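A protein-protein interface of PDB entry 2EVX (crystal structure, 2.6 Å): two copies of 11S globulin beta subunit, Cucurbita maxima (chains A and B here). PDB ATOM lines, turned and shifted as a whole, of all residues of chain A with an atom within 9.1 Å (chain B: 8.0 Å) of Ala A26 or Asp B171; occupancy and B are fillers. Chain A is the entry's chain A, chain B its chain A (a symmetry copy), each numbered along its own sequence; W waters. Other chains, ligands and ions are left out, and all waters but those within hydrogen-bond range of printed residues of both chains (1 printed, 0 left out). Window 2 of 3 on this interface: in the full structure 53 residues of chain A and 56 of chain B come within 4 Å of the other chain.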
ATOM      1  N   ALA A  26      21.965   0.511  12.793  1.00  0.00           N
ATOM      2  CA  ALA A  26      20.481   0.340  12.797  1.00  0.00           C
ATOM      3  C   ALA A  26      19.820   1.205  11.715  1.00  0.00           C
ATOM      4  O   ALA A  26      19.744   2.429  11.835  1.00  0.00           O
ATOM      5  CB  ALA A  26      19.923   0.698  14.175  1.00  0.00           C
ATOM      6  N   CYS A  27      19.345   0.551  10.661  1.00  0.00           N
ATOM      7  CA  CYS A  27      18.688   1.222   9.545  1.00  0.00           C
ATOM      8  C   CYS A  27      17.176   1.224   9.712  1.00  0.00           C
ATOM      9  O   CYS A  27      16.571   0.178   9.903  1.00  0.00           O
ATOM     10  CB  CYS A  27      19.036   0.506   8.246  1.00  0.00           C
ATOM     11  SG  CYS A  27      20.646   0.916   7.496  1.00  0.00           S
ATOM     12  N   ARG A  28      16.558   2.395   9.634  1.00  0.00           N
ATOM     13  CA  ARG A  28      15.105   2.475   9.769  1.00  0.00           C
ATOM     14  C   ARG A  28      14.424   2.353   8.408  1.00  0.00           C
ATOM     15  O   ARG A  28      14.216   3.348   7.706  1.00  0.00           O
ATOM     16  CB  ARG A  28      14.694   3.786  10.448  1.00  0.00           C
ATOM     17  CG  ARG A  28      15.065   3.860  11.922  1.00  0.00           C
ATOM     18  CD  ARG A  28      14.109   4.773  12.701  1.00  0.00           C
ATOM     19  NE  ARG A  28      14.160   6.171  12.264  1.00  0.00           N
ATOM     20  CZ  ARG A  28      13.366   7.133  12.732  1.00  0.00           C
ATOM     21  NH1 ARG A  28      12.452   6.850  13.653  1.00  0.00           N
ATOM     22  NH2 ARG A  28      13.487   8.381  12.285  1.00  0.00           N
ATOM     23  N   LEU A  29      14.087   1.120   8.045  1.00  0.00           N
ATOM     24  CA  LEU A  29      13.446   0.853   6.775  1.00  0.00           C
ATOM     25  C   LEU A  29      12.053   0.322   6.954  1.00  0.00           C
ATOM     26  O   LEU A  29      11.630  -0.563   6.219  1.00  0.00           O
ATOM     27  CB  LEU A  29      14.235  -0.168   5.964  1.00  0.00           C
ATOM     28  CG  LEU A  29      15.685   0.108   5.603  1.00  0.00           C
ATOM     29  CD1 LEU A  29      15.906   1.595   5.433  1.00  0.00           C
ATOM     30  CD2 LEU A  29      16.558  -0.442   6.681  1.00  0.00           C
ATOM     31  N   ASP A  56      15.614   8.531   6.232  1.00  0.00           N
ATOM     32  CA  ASP A  56      16.077   7.248   6.750  1.00  0.00           C
ATOM     33  C   ASP A  56      16.578   6.272   5.678  1.00  0.00           C
ATOM     34  O   ASP A  56      17.652   5.680   5.839  1.00  0.00           O
ATOM     35  CB  ASP A  56      14.983   6.603   7.602  1.00  0.00           C
ATOM     36  CG  ASP A  56      14.743   7.354   8.914  1.00  0.00           C
ATOM     37  OD1 ASP A  56      13.706   7.099   9.564  1.00  0.00           O
ATOM     38  OD2 ASP A  56      15.590   8.196   9.303  1.00  0.00           O
ATOM     39  N   GLU A  57      15.825   6.105   4.591  1.00  0.00           N
ATOM     40  CA  GLU A  57      16.247   5.208   3.508  1.00  0.00           C
ATOM     41  C   GLU A  57      17.615   5.654   2.978  1.00  0.00           C
ATOM     42  O   GLU A  57      18.578   4.878   2.968  1.00  0.00           O
ATOM     43  CB  GLU A  57      15.267   5.229   2.315  1.00  0.00           C
ATOM     44  CG  GLU A  57      13.805   4.885   2.590  1.00  0.00           C
ATOM     45  CD  GLU A  57      13.008   6.057   3.142  1.00  0.00           C
ATOM     46  OE1 GLU A  57      13.131   6.339   4.352  1.00  0.00           O
ATOM     47  OE2 GLU A  57      12.268   6.695   2.365  1.00  0.00           O
ATOM     48  N   GLN A  59      19.868   7.708   4.171  1.00  0.00           N
ATOM     49  CA  GLN A  59      20.915   7.648   5.175  1.00  0.00           C
ATOM     50  C   GLN A  59      21.474   6.229   5.261  1.00  0.00           C
ATOM     51  O   GLN A  59      22.686   6.024   5.294  1.00  0.00           O
ATOM     52  CB  GLN A  59      20.351   8.083   6.528  1.00  0.00           C
ATOM     53  CG  GLN A  59      21.238   9.021   7.300  1.00  0.00           C
ATOM     54  CD  GLN A  59      20.670   9.359   8.669  1.00  0.00           C
ATOM     55  OE1 GLN A  59      19.509   9.757   8.794  1.00  0.00           O
ATOM     56  NE2 GLN A  59      21.492   9.206   9.707  1.00  0.00           N
ATOM     57  N   CYS A  60      20.586   5.247   5.272  1.00  0.00           N
ATOM     58  CA  CYS A  60      20.992   3.855   5.360  1.00  0.00           C
ATOM     59  C   CYS A  60      21.832   3.395   4.176  1.00  0.00           C
ATOM     60  O   CYS A  60      22.805   2.659   4.346  1.00  0.00           O
ATOM     61  CB  CYS A  60      19.757   2.972   5.466  1.00  0.00           C
ATOM     62  SG  CYS A  60      20.158   1.207   5.532  1.00  0.00           S
ATOM     63  N   ALA A  61      21.447   3.818   2.976  1.00  0.00           N
ATOM     64  CA  ALA A  61      22.154   3.436   1.760  1.00  0.00           C
ATOM     65  C   ALA A  61      23.296   4.390   1.402  1.00  0.00           C
ATOM     66  O   ALA A  61      24.131   4.076   0.555  1.00  0.00           O
ATOM     67  CB  ALA A  61      21.175   3.344   0.608  1.00  0.00           C
ATOM     68  N   ARG A 164      28.591   6.273   0.663  1.00  0.00           N
ATOM     69  CA  ARG A 164      29.127   5.091   1.310  1.00  0.00           C
ATOM     70  C   ARG A 164      29.885   4.276   0.273  1.00  0.00           C
ATOM     71  O   ARG A 164      30.021   3.059   0.369  1.00  0.00           O
ATOM     72  CB  ARG A 164      28.008   4.263   1.929  1.00  0.00           C
ATOM     73  CG  ARG A 164      27.487   4.833   3.237  1.00  0.00           C
ATOM     74  CD  ARG A 164      26.383   3.950   3.820  1.00  0.00           C
ATOM     75  NE  ARG A 164      25.778   4.557   5.003  1.00  0.00           N
ATOM     76  CZ  ARG A 164      26.367   4.624   6.191  1.00  0.00           C
ATOM     77  NH1 ARG A 164      25.742   5.204   7.207  1.00  0.00           N
ATOM     78  NH2 ARG A 164      27.570   4.094   6.366  1.00  0.00           N
ATOM     79  N   HIS A 344      20.972  -1.575  -3.458  1.00  0.00           N
ATOM     80  CA  HIS A 344      19.776  -0.800  -3.223  1.00  0.00           C
ATOM     81  C   HIS A 344      19.322  -0.333  -4.614  1.00  0.00           C
ATOM     82  O   HIS A 344      20.018  -0.544  -5.612  1.00  0.00           O
ATOM     83  CB  HIS A 344      20.099   0.412  -2.347  1.00  0.00           C
ATOM     84  CG  HIS A 344      20.747   0.064  -1.041  1.00  0.00           C
ATOM     85  ND1 HIS A 344      20.126  -0.708  -0.082  1.00  0.00           N
ATOM     86  CD2 HIS A 344      21.958   0.394  -0.531  1.00  0.00           C
ATOM     87  CE1 HIS A 344      20.924  -0.836   0.963  1.00  0.00           C
ATOM     88  NE2 HIS A 344      22.042  -0.176   0.716  1.00  0.00           N
ATOM     89  N   ASN A 361      11.520  -8.195   5.346  1.00  0.00           N
ATOM     90  CA  ASN A 361      11.741  -9.570   5.781  1.00  0.00           C
ATOM     91  C   ASN A 361      10.745 -10.043   6.843  1.00  0.00           C
ATOM     92  O   ASN A 361      10.717 -11.228   7.194  1.00  0.00           O
ATOM     93  CB  ASN A 361      13.170  -9.716   6.296  1.00  0.00           C
ATOM     94  CG  ASN A 361      13.490  -8.731   7.400  1.00  0.00           C
ATOM     95  OD1 ASN A 361      13.548  -9.099   8.572  1.00  0.00           O
ATOM     96  ND2 ASN A 361      13.684  -7.468   7.033  1.00  0.00           N
ATOM     97  N   PRO A 380      15.156  -0.656  -0.592  1.00  0.00           N
ATOM     98  CA  PRO A 380      16.263  -1.347   0.079  1.00  0.00           C
ATOM     99  C   PRO A 380      16.620  -2.716  -0.503  1.00  0.00           C
ATOM    100  O   PRO A 380      15.763  -3.443  -1.009  1.00  0.00           O
ATOM    101  CB  PRO A 380      15.775  -1.452   1.521  1.00  0.00           C
ATOM    102  CG  PRO A 380      14.946  -0.197   1.671  1.00  0.00           C
ATOM    103  CD  PRO A 380      14.157  -0.187   0.385  1.00  0.00           C
ATOM    104  N   GLN A 381      17.900  -3.054  -0.408  1.00  0.00           N
ATOM    105  CA  GLN A 381      18.424  -4.328  -0.879  1.00  0.00           C
ATOM    106  C   GLN A 381      17.657  -5.516  -0.252  1.00  0.00           C
ATOM    107  O   GLN A 381      17.447  -5.561   0.958  1.00  0.00           O
ATOM    108  CB  GLN A 381      19.909  -4.396  -0.524  1.00  0.00           C
ATOM    109  CG  GLN A 381      20.602  -5.711  -0.833  1.00  0.00           C
ATOM    110  CD  GLN A 381      21.937  -5.823  -0.121  1.00  0.00           C
ATOM    111  OE1 GLN A 381      22.655  -6.810  -0.277  1.00  0.00           O
ATOM    112  NE2 GLN A 381      22.274  -4.806   0.675  1.00  0.00           N
ATOM    113  N   ASN A 382      17.244  -6.463  -1.091  1.00  0.00           N
ATOM    114  CA  ASN A 382      16.509  -7.656  -0.671  1.00  0.00           C
ATOM    115  C   ASN A 382      15.009  -7.438  -0.446  1.00  0.00           C
ATOM    116  O   ASN A 382      14.254  -8.407  -0.320  1.00  0.00           O
ATOM    117  CB  ASN A 382      17.101  -8.256   0.607  1.00  0.00           C
ATOM    118  CG  ASN A 382      18.549  -8.660   0.454  1.00  0.00           C
ATOM    119  OD1 ASN A 382      18.903  -9.406  -0.452  1.00  0.00           O
ATOM    120  ND2 ASN A 382      19.398  -8.176   1.358  1.00  0.00           N
ATOM    121  N   PHE A 383      14.572  -6.185  -0.376  1.00  0.00           N
ATOM    122  CA  PHE A 383      13.156  -5.919  -0.168  1.00  0.00           C
ATOM    123  C   PHE A 383      12.375  -6.276  -1.417  1.00  0.00           C
ATOM    124  O   PHE A 383      12.731  -5.863  -2.515  1.00  0.00           O
ATOM    125  CB  PHE A 383      12.912  -4.449   0.179  1.00  0.00           C
ATOM    126  CG  PHE A 383      13.286  -4.088   1.585  1.00  0.00           C
ATOM    127  CD1 PHE A 383      12.557  -3.126   2.281  1.00  0.00           C
ATOM    128  CD2 PHE A 383      14.346  -4.721   2.224  1.00  0.00           C
ATOM    129  CE1 PHE A 383      12.873  -2.801   3.594  1.00  0.00           C
ATOM    130  CE2 PHE A 383      14.671  -4.409   3.532  1.00  0.00           C
ATOM    131  CZ  PHE A 383      13.931  -3.444   4.223  1.00  0.00           C
ATOM    132  N   ASN B  82      20.275 -11.273   3.974  1.00  0.00           N
ATOM    133  CA  ASN B  82      21.061 -10.133   3.534  1.00  0.00           C
ATOM    134  C   ASN B  82      22.541 -10.377   3.814  1.00  0.00           C
ATOM    135  O   ASN B  82      23.380  -9.518   3.556  1.00  0.00           O
ATOM    136  CB  ASN B  82      20.617  -8.875   4.277  1.00  0.00           C
ATOM    137  CG  ASN B  82      20.754  -9.009   5.801  1.00  0.00           C
ATOM    138  OD1 ASN B  82      21.076  -8.041   6.488  1.00  0.00           O
ATOM    139  ND2 ASN B  82      20.499 -10.205   6.327  1.00  0.00           N
ATOM    140  N   ALA B  83      22.862 -11.546   4.346  1.00  0.00           N
ATOM    141  CA  ALA B  83      24.243 -11.863   4.667  1.00  0.00           C
ATOM    142  C   ALA B  83      24.629 -13.268   4.247  1.00  0.00           C
ATOM    143  O   ALA B  83      23.813 -14.183   4.274  1.00  0.00           O
ATOM    144  CB  ALA B  83      24.469 -11.699   6.148  1.00  0.00           C
ATOM    145  N   ASP B 162      27.492 -13.756   8.587  1.00  0.00           N
ATOM    146  CA  ASP B 162      28.291 -12.566   8.825  1.00  0.00           C
ATOM    147  C   ASP B 162      27.538 -11.368   8.281  1.00  0.00           C
ATOM    148  O   ASP B 162      27.254 -11.311   7.092  1.00  0.00           O
ATOM    149  CB  ASP B 162      29.650 -12.667   8.128  1.00  0.00           C
ATOM    150  CG  ASP B 162      30.655 -11.667   8.678  1.00  0.00           C
ATOM    151  OD1 ASP B 162      30.382 -10.451   8.637  1.00  0.00           O
ATOM    152  OD2 ASP B 162      31.719 -12.098   9.169  1.00  0.00           O
ATOM    153  N   THR B 163      27.218 -10.411   9.145  1.00  0.00           N
ATOM    154  CA  THR B 163      26.497  -9.223   8.715  1.00  0.00           C
ATOM    155  C   THR B 163      27.444  -8.098   8.324  1.00  0.00           C
ATOM    156  O   THR B 163      27.055  -7.168   7.632  1.00  0.00           O
ATOM    157  CB  THR B 163      25.555  -8.714   9.804  1.00  0.00           C
ATOM    158  OG1 THR B 163      26.320  -8.321  10.951  1.00  0.00           O
ATOM    159  CG2 THR B 163      24.575  -9.806  10.204  1.00  0.00           C
ATOM    160  N   ARG B 164      28.688  -8.161   8.769  1.00  0.00           N
ATOM    161  CA  ARG B 164      29.627  -7.123   8.391  1.00  0.00           C
ATOM    162  C   ARG B 164      30.356  -7.568   7.132  1.00  0.00           C
ATOM    163  O   ARG B 164      31.487  -7.175   6.858  1.00  0.00           O
ATOM    164  CB  ARG B 164      30.616  -6.857   9.518  1.00  0.00           C
ATOM    165  CG  ARG B 164      30.037  -6.024  10.647  1.00  0.00           C
ATOM    166  CD  ARG B 164      31.080  -5.772  11.737  1.00  0.00           C
ATOM    167  NE  ARG B 164      30.499  -5.093  12.892  1.00  0.00           N
ATOM    168  CZ  ARG B 164      30.157  -3.810  12.908  1.00  0.00           C
ATOM    169  NH1 ARG B 164      29.626  -3.280  14.002  1.00  0.00           N
ATOM    170  NH2 ARG B 164      30.366  -3.054  11.837  1.00  0.00           N
ATOM    171  N   ASN B 165      29.681  -8.398   6.355  1.00  0.00           N
ATOM    172  CA  ASN B 165      30.241  -8.909   5.124  1.00  0.00           C
ATOM    173  C   ASN B 165      30.000  -7.905   3.988  1.00  0.00           C
ATOM    174  O   ASN B 165      28.944  -7.260   3.914  1.00  0.00           O
ATOM    175  CB  ASN B 165      29.587 -10.255   4.813  1.00  0.00           C
ATOM    176  CG  ASN B 165      30.259 -10.984   3.678  1.00  0.00           C
ATOM    177  OD1 ASN B 165      29.987 -10.729   2.498  1.00  0.00           O
ATOM    178  ND2 ASN B 165      31.155 -11.903   4.026  1.00  0.00           N
ATOM    179  N   ASN B 168      26.477  -7.525   2.296  1.00  0.00           N
ATOM    180  CA  ASN B 168      25.299  -6.893   2.894  1.00  0.00           C
ATOM    181  C   ASN B 168      25.439  -5.376   2.933  1.00  0.00           C
ATOM    182  O   ASN B 168      26.318  -4.852   3.605  1.00  0.00           O
ATOM    183  CB  ASN B 168      25.079  -7.429   4.309  1.00  0.00           C
ATOM    184  CG  ASN B 168      24.160  -6.554   5.128  1.00  0.00           C
ATOM    185  OD1 ASN B 168      23.174  -6.024   4.624  1.00  0.00           O
ATOM    186  ND2 ASN B 168      24.473  -6.411   6.402  1.00  0.00           N
ATOM    187  N   GLN B 169      24.561  -4.676   2.223  1.00  0.00           N
ATOM    188  CA  GLN B 169      24.615  -3.217   2.159  1.00  0.00           C
ATOM    189  C   GLN B 169      23.676  -2.477   3.109  1.00  0.00           C
ATOM    190  O   GLN B 169      23.613  -1.247   3.089  1.00  0.00           O
ATOM    191  CB  GLN B 169      24.359  -2.751   0.718  1.00  0.00           C
ATOM    192  CG  GLN B 169      25.579  -2.871  -0.202  1.00  0.00           C
ATOM    193  CD  GLN B 169      25.292  -2.492  -1.653  1.00  0.00           C
ATOM    194  OE1 GLN B 169      24.599  -1.515  -1.924  1.00  0.00           O
ATOM    195  NE2 GLN B 169      25.843  -3.261  -2.590  1.00  0.00           N
ATOM    196  N   ILE B 170      22.954  -3.209   3.947  1.00  0.00           N
ATOM    197  CA  ILE B 170      22.041  -2.565   4.879  1.00  0.00           C
ATOM    198  C   ILE B 170      22.731  -2.213   6.197  1.00  0.00           C
ATOM    199  O   ILE B 170      23.402  -1.186   6.287  1.00  0.00           O
ATOM    200  CB  ILE B 170      20.823  -3.457   5.150  1.00  0.00           C
ATOM    201  CG1 ILE B 170      20.113  -3.761   3.831  1.00  0.00           C
ATOM    202  CG2 ILE B 170      19.874  -2.767   6.118  1.00  0.00           C
ATOM    203  CD1 ILE B 170      19.137  -4.924   3.917  1.00  0.00           C
ATOM    204  N   ASP B 171      22.565  -3.059   7.211  1.00  0.00           N
ATOM    205  CA  ASP B 171      23.167  -2.835   8.527  1.00  0.00           C
ATOM    206  C   ASP B 171      23.611  -4.166   9.138  1.00  0.00           C
ATOM    207  O   ASP B 171      23.208  -5.228   8.667  1.00  0.00           O
ATOM    208  CB  ASP B 171      22.164  -2.135   9.456  1.00  0.00           C
ATOM    209  CG  ASP B 171      20.885  -2.928   9.646  1.00  0.00           C
ATOM    210  OD1 ASP B 171      19.968  -2.404  10.311  1.00  0.00           O
ATOM    211  OD2 ASP B 171      20.788  -4.066   9.137  1.00  0.00           O
ATOM    212  N   PRO B 172      24.431  -4.124  10.205  1.00  0.00           N
ATOM    213  CA  PRO B 172      24.935  -5.335  10.876  1.00  0.00           C
ATOM    214  C   PRO B 172      23.863  -6.211  11.496  1.00  0.00           C
ATOM    215  O   PRO B 172      24.152  -7.038  12.356  1.00  0.00           O
ATOM    216  CB  PRO B 172      25.899  -4.779  11.920  1.00  0.00           C
ATOM    217  CG  PRO B 172      25.259  -3.489  12.290  1.00  0.00           C
ATOM    218  CD  PRO B 172      24.843  -2.917  10.946  1.00  0.00           C
ATOM    219  N   TYR B 173      22.630  -6.042  11.039  1.00  0.00           N
ATOM    220  CA  TYR B 173      21.512  -6.814  11.558  1.00  0.00           C
ATOM    221  C   TYR B 173      20.958  -7.819  10.533  1.00  0.00           C
ATOM    222  O   TYR B 173      20.535  -7.474   9.432  1.00  0.00           O
ATOM    223  CB  TYR B 173      20.434  -5.813  12.053  1.00  0.00           C
ATOM    224  CG  TYR B 173      18.964  -6.096  11.751  1.00  0.00           C
ATOM    225  CD1 TYR B 173      18.149  -5.098  11.170  1.00  0.00           C
ATOM    226  CD2 TYR B 173      18.369  -7.338  12.071  1.00  0.00           C
ATOM    227  CE1 TYR B 173      16.762  -5.330  10.913  1.00  0.00           C
ATOM    228  CE2 TYR B 173      16.983  -7.584  11.819  1.00  0.00           C
ATOM    229  CZ  TYR B 173      16.192  -6.575  11.241  1.00  0.00           C
ATOM    230  OH  TYR B 173      14.858  -6.805  10.994  1.00  0.00           O
ATOM    231  N   LEU B 174      20.998  -9.082  10.929  1.00  0.00           N
ATOM    232  CA  LEU B 174      20.559 -10.205  10.119  1.00  0.00           C
ATOM    233  C   LEU B 174      19.064 -10.239   9.808  1.00  0.00           C
ATOM    234  O   LEU B 174      18.228 -10.048  10.689  1.00  0.00           O
ATOM    235  CB  LEU B 174      20.975 -11.495  10.816  1.00  0.00           C
ATOM    236  CG  LEU B 174      20.728 -12.805  10.087  1.00  0.00           C
ATOM    237  CD1 LEU B 174      21.434 -12.809   8.734  1.00  0.00           C
ATOM    238  CD2 LEU B 174      21.233 -13.928  10.965  1.00  0.00           C
ATOM    239  N   ARG B 175      18.743 -10.513   8.544  1.00  0.00           N
ATOM    240  CA  ARG B 175      17.368 -10.570   8.076  1.00  0.00           C
ATOM    241  C   ARG B 175      17.178 -11.787   7.173  1.00  0.00           C
ATOM    242  O   ARG B 175      17.994 -12.048   6.296  1.00  0.00           O
ATOM    243  CB  ARG B 175      17.026  -9.305   7.274  1.00  0.00           C
ATOM    244  CG  ARG B 175      17.115  -7.971   8.019  1.00  0.00           C
ATOM    245  CD  ARG B 175      16.841  -6.817   7.066  1.00  0.00           C
ATOM    246  NE  ARG B 175      16.898  -5.485   7.667  1.00  0.00           N
ATOM    247  CZ  ARG B 175      15.827  -4.750   7.987  1.00  0.00           C
ATOM    248  NH1 ARG B 175      14.600  -5.209   7.777  1.00  0.00           N
ATOM    249  NH2 ARG B 175      15.975  -3.531   8.498  1.00  0.00           N
ATOM    250  N   ARG B 188      16.706 -12.953  14.587  1.00  0.00           N
ATOM    251  CA  ARG B 188      17.174 -11.665  15.082  1.00  0.00           C
ATOM    252  C   ARG B 188      16.153 -10.995  16.018  1.00  0.00           C
ATOM    253  O   ARG B 188      16.484 -10.040  16.731  1.00  0.00           O
ATOM    254  CB  ARG B 188      17.495 -10.739  13.907  1.00  0.00           C
ATOM    255  CG  ARG B 188      18.440  -9.626  14.283  1.00  0.00           C
ATOM    256  CD  ARG B 188      19.690 -10.170  14.959  1.00  0.00           C
ATOM    257  NE  ARG B 188      20.746  -9.165  15.020  1.00  0.00           N
ATOM    258  CZ  ARG B 188      21.728  -9.062  14.132  1.00  0.00           C
ATOM    259  NH1 ARG B 188      21.794  -9.909  13.117  1.00  0.00           N
ATOM    260  NH2 ARG B 188      22.639  -8.106  14.252  1.00  0.00           N
HETATM  261  O   HOH W   1      14.248  -1.230   9.366  1.00  0.00           O
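The backbone NH of Cys A27 is in hydrogen-bond range of the side-chain carboxylate of Asp B171 (3.0 Å).
ND2 of Asn A361 lies close to NH1 of Arg B175 (2.5 Å).
NE2 of His A344 lies within hydrogen-bond range of O of Gln B169 (3.0 Å).
The side-chain amide nitrogen (NE2) of Gln A381 lies close to the backbone NH (N) of Gln B169 (2.8 Å).
The side-chain sulfur (SG) of Cys A27 lies close to the backbone carbonyl oxygen (O) of Ile B170, 3.7 Å away.
The side-chain amide oxygen (OD1) of Asn B82 lies close to the side-chain amide oxygen (OD1) of Asn B168 (3.5 Å).
The side-chain carboxylate (OD2) of Asp B171 lies close to the backbone NH (N) of Tyr B173 (3.3 Å).
The backbone NH of Gln A381 is in hydrogen-bond range of a ring nitrogen (ND1) of His A344 (3.3 Å).
The backbone NH (N) of Arg B175 lies close to the side-chain amide nitrogen (ND2) of Asn B82 (2.8 Å).
The backbone carbonyl oxygen (O) of Thr B163 lies within hydrogen-bond range of the side-chain amide nitrogen (ND2) of Asn B168.
The side-chain sulfur of Cys A27 forms a disulfide with the side-chain sulfur of Cys A60, 2.0 Å away.
Among the printed residues, merely in contact across the chains: Asn A382 with Asn B82, Gln A381 with Ile B170, Asn A361 with Tyr B173, Leu A29 with Arg B175, Ala A26 with Asp B171 and Gln A381 with Asn B168.
Of chain B, only Asp B171 comes within 4 Å of Ala A26.
No residue of chain A comes within 4 Å of Pro B172.
Printed residues of chain A within 4 Å of Asn B82: Asn A382.
Of the printed residues of chain B, Gln A381 touches Asn B168, Gln B169 and Ile B170.
Printed residues of chain B within 4 Å of Asn A382: Asn B82 (3.2 Å).
Asp B162 touches none of the printed residues of chain A.
The nearest residue of chain A that does not touch Asp B171 is Cys A60 (5.2 Å).
The nearest printed residue of chain B that does not touch Gln A381 is Asn B82 (4.7 Å).
Hydrophobic or aromatic side chains of chain B within 4 Å of the printed part of chain A: Ile B170 and Tyr B173.
Among the printed residues, 11 pairs touch across the chains.
Position printed for both chains: 164.
Of the 11 pairs that touch across the chains among the printed residues, none has its exchanged pair printed and touching as well.
Water W1 lies within hydrogen-bond range of the backbone NH of Leu A29 (2.7 Å), the backbone carbonyl oxygen of Cys A27 (2.8 Å) and the guanidinium group of Arg B175 (3.0 Å).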
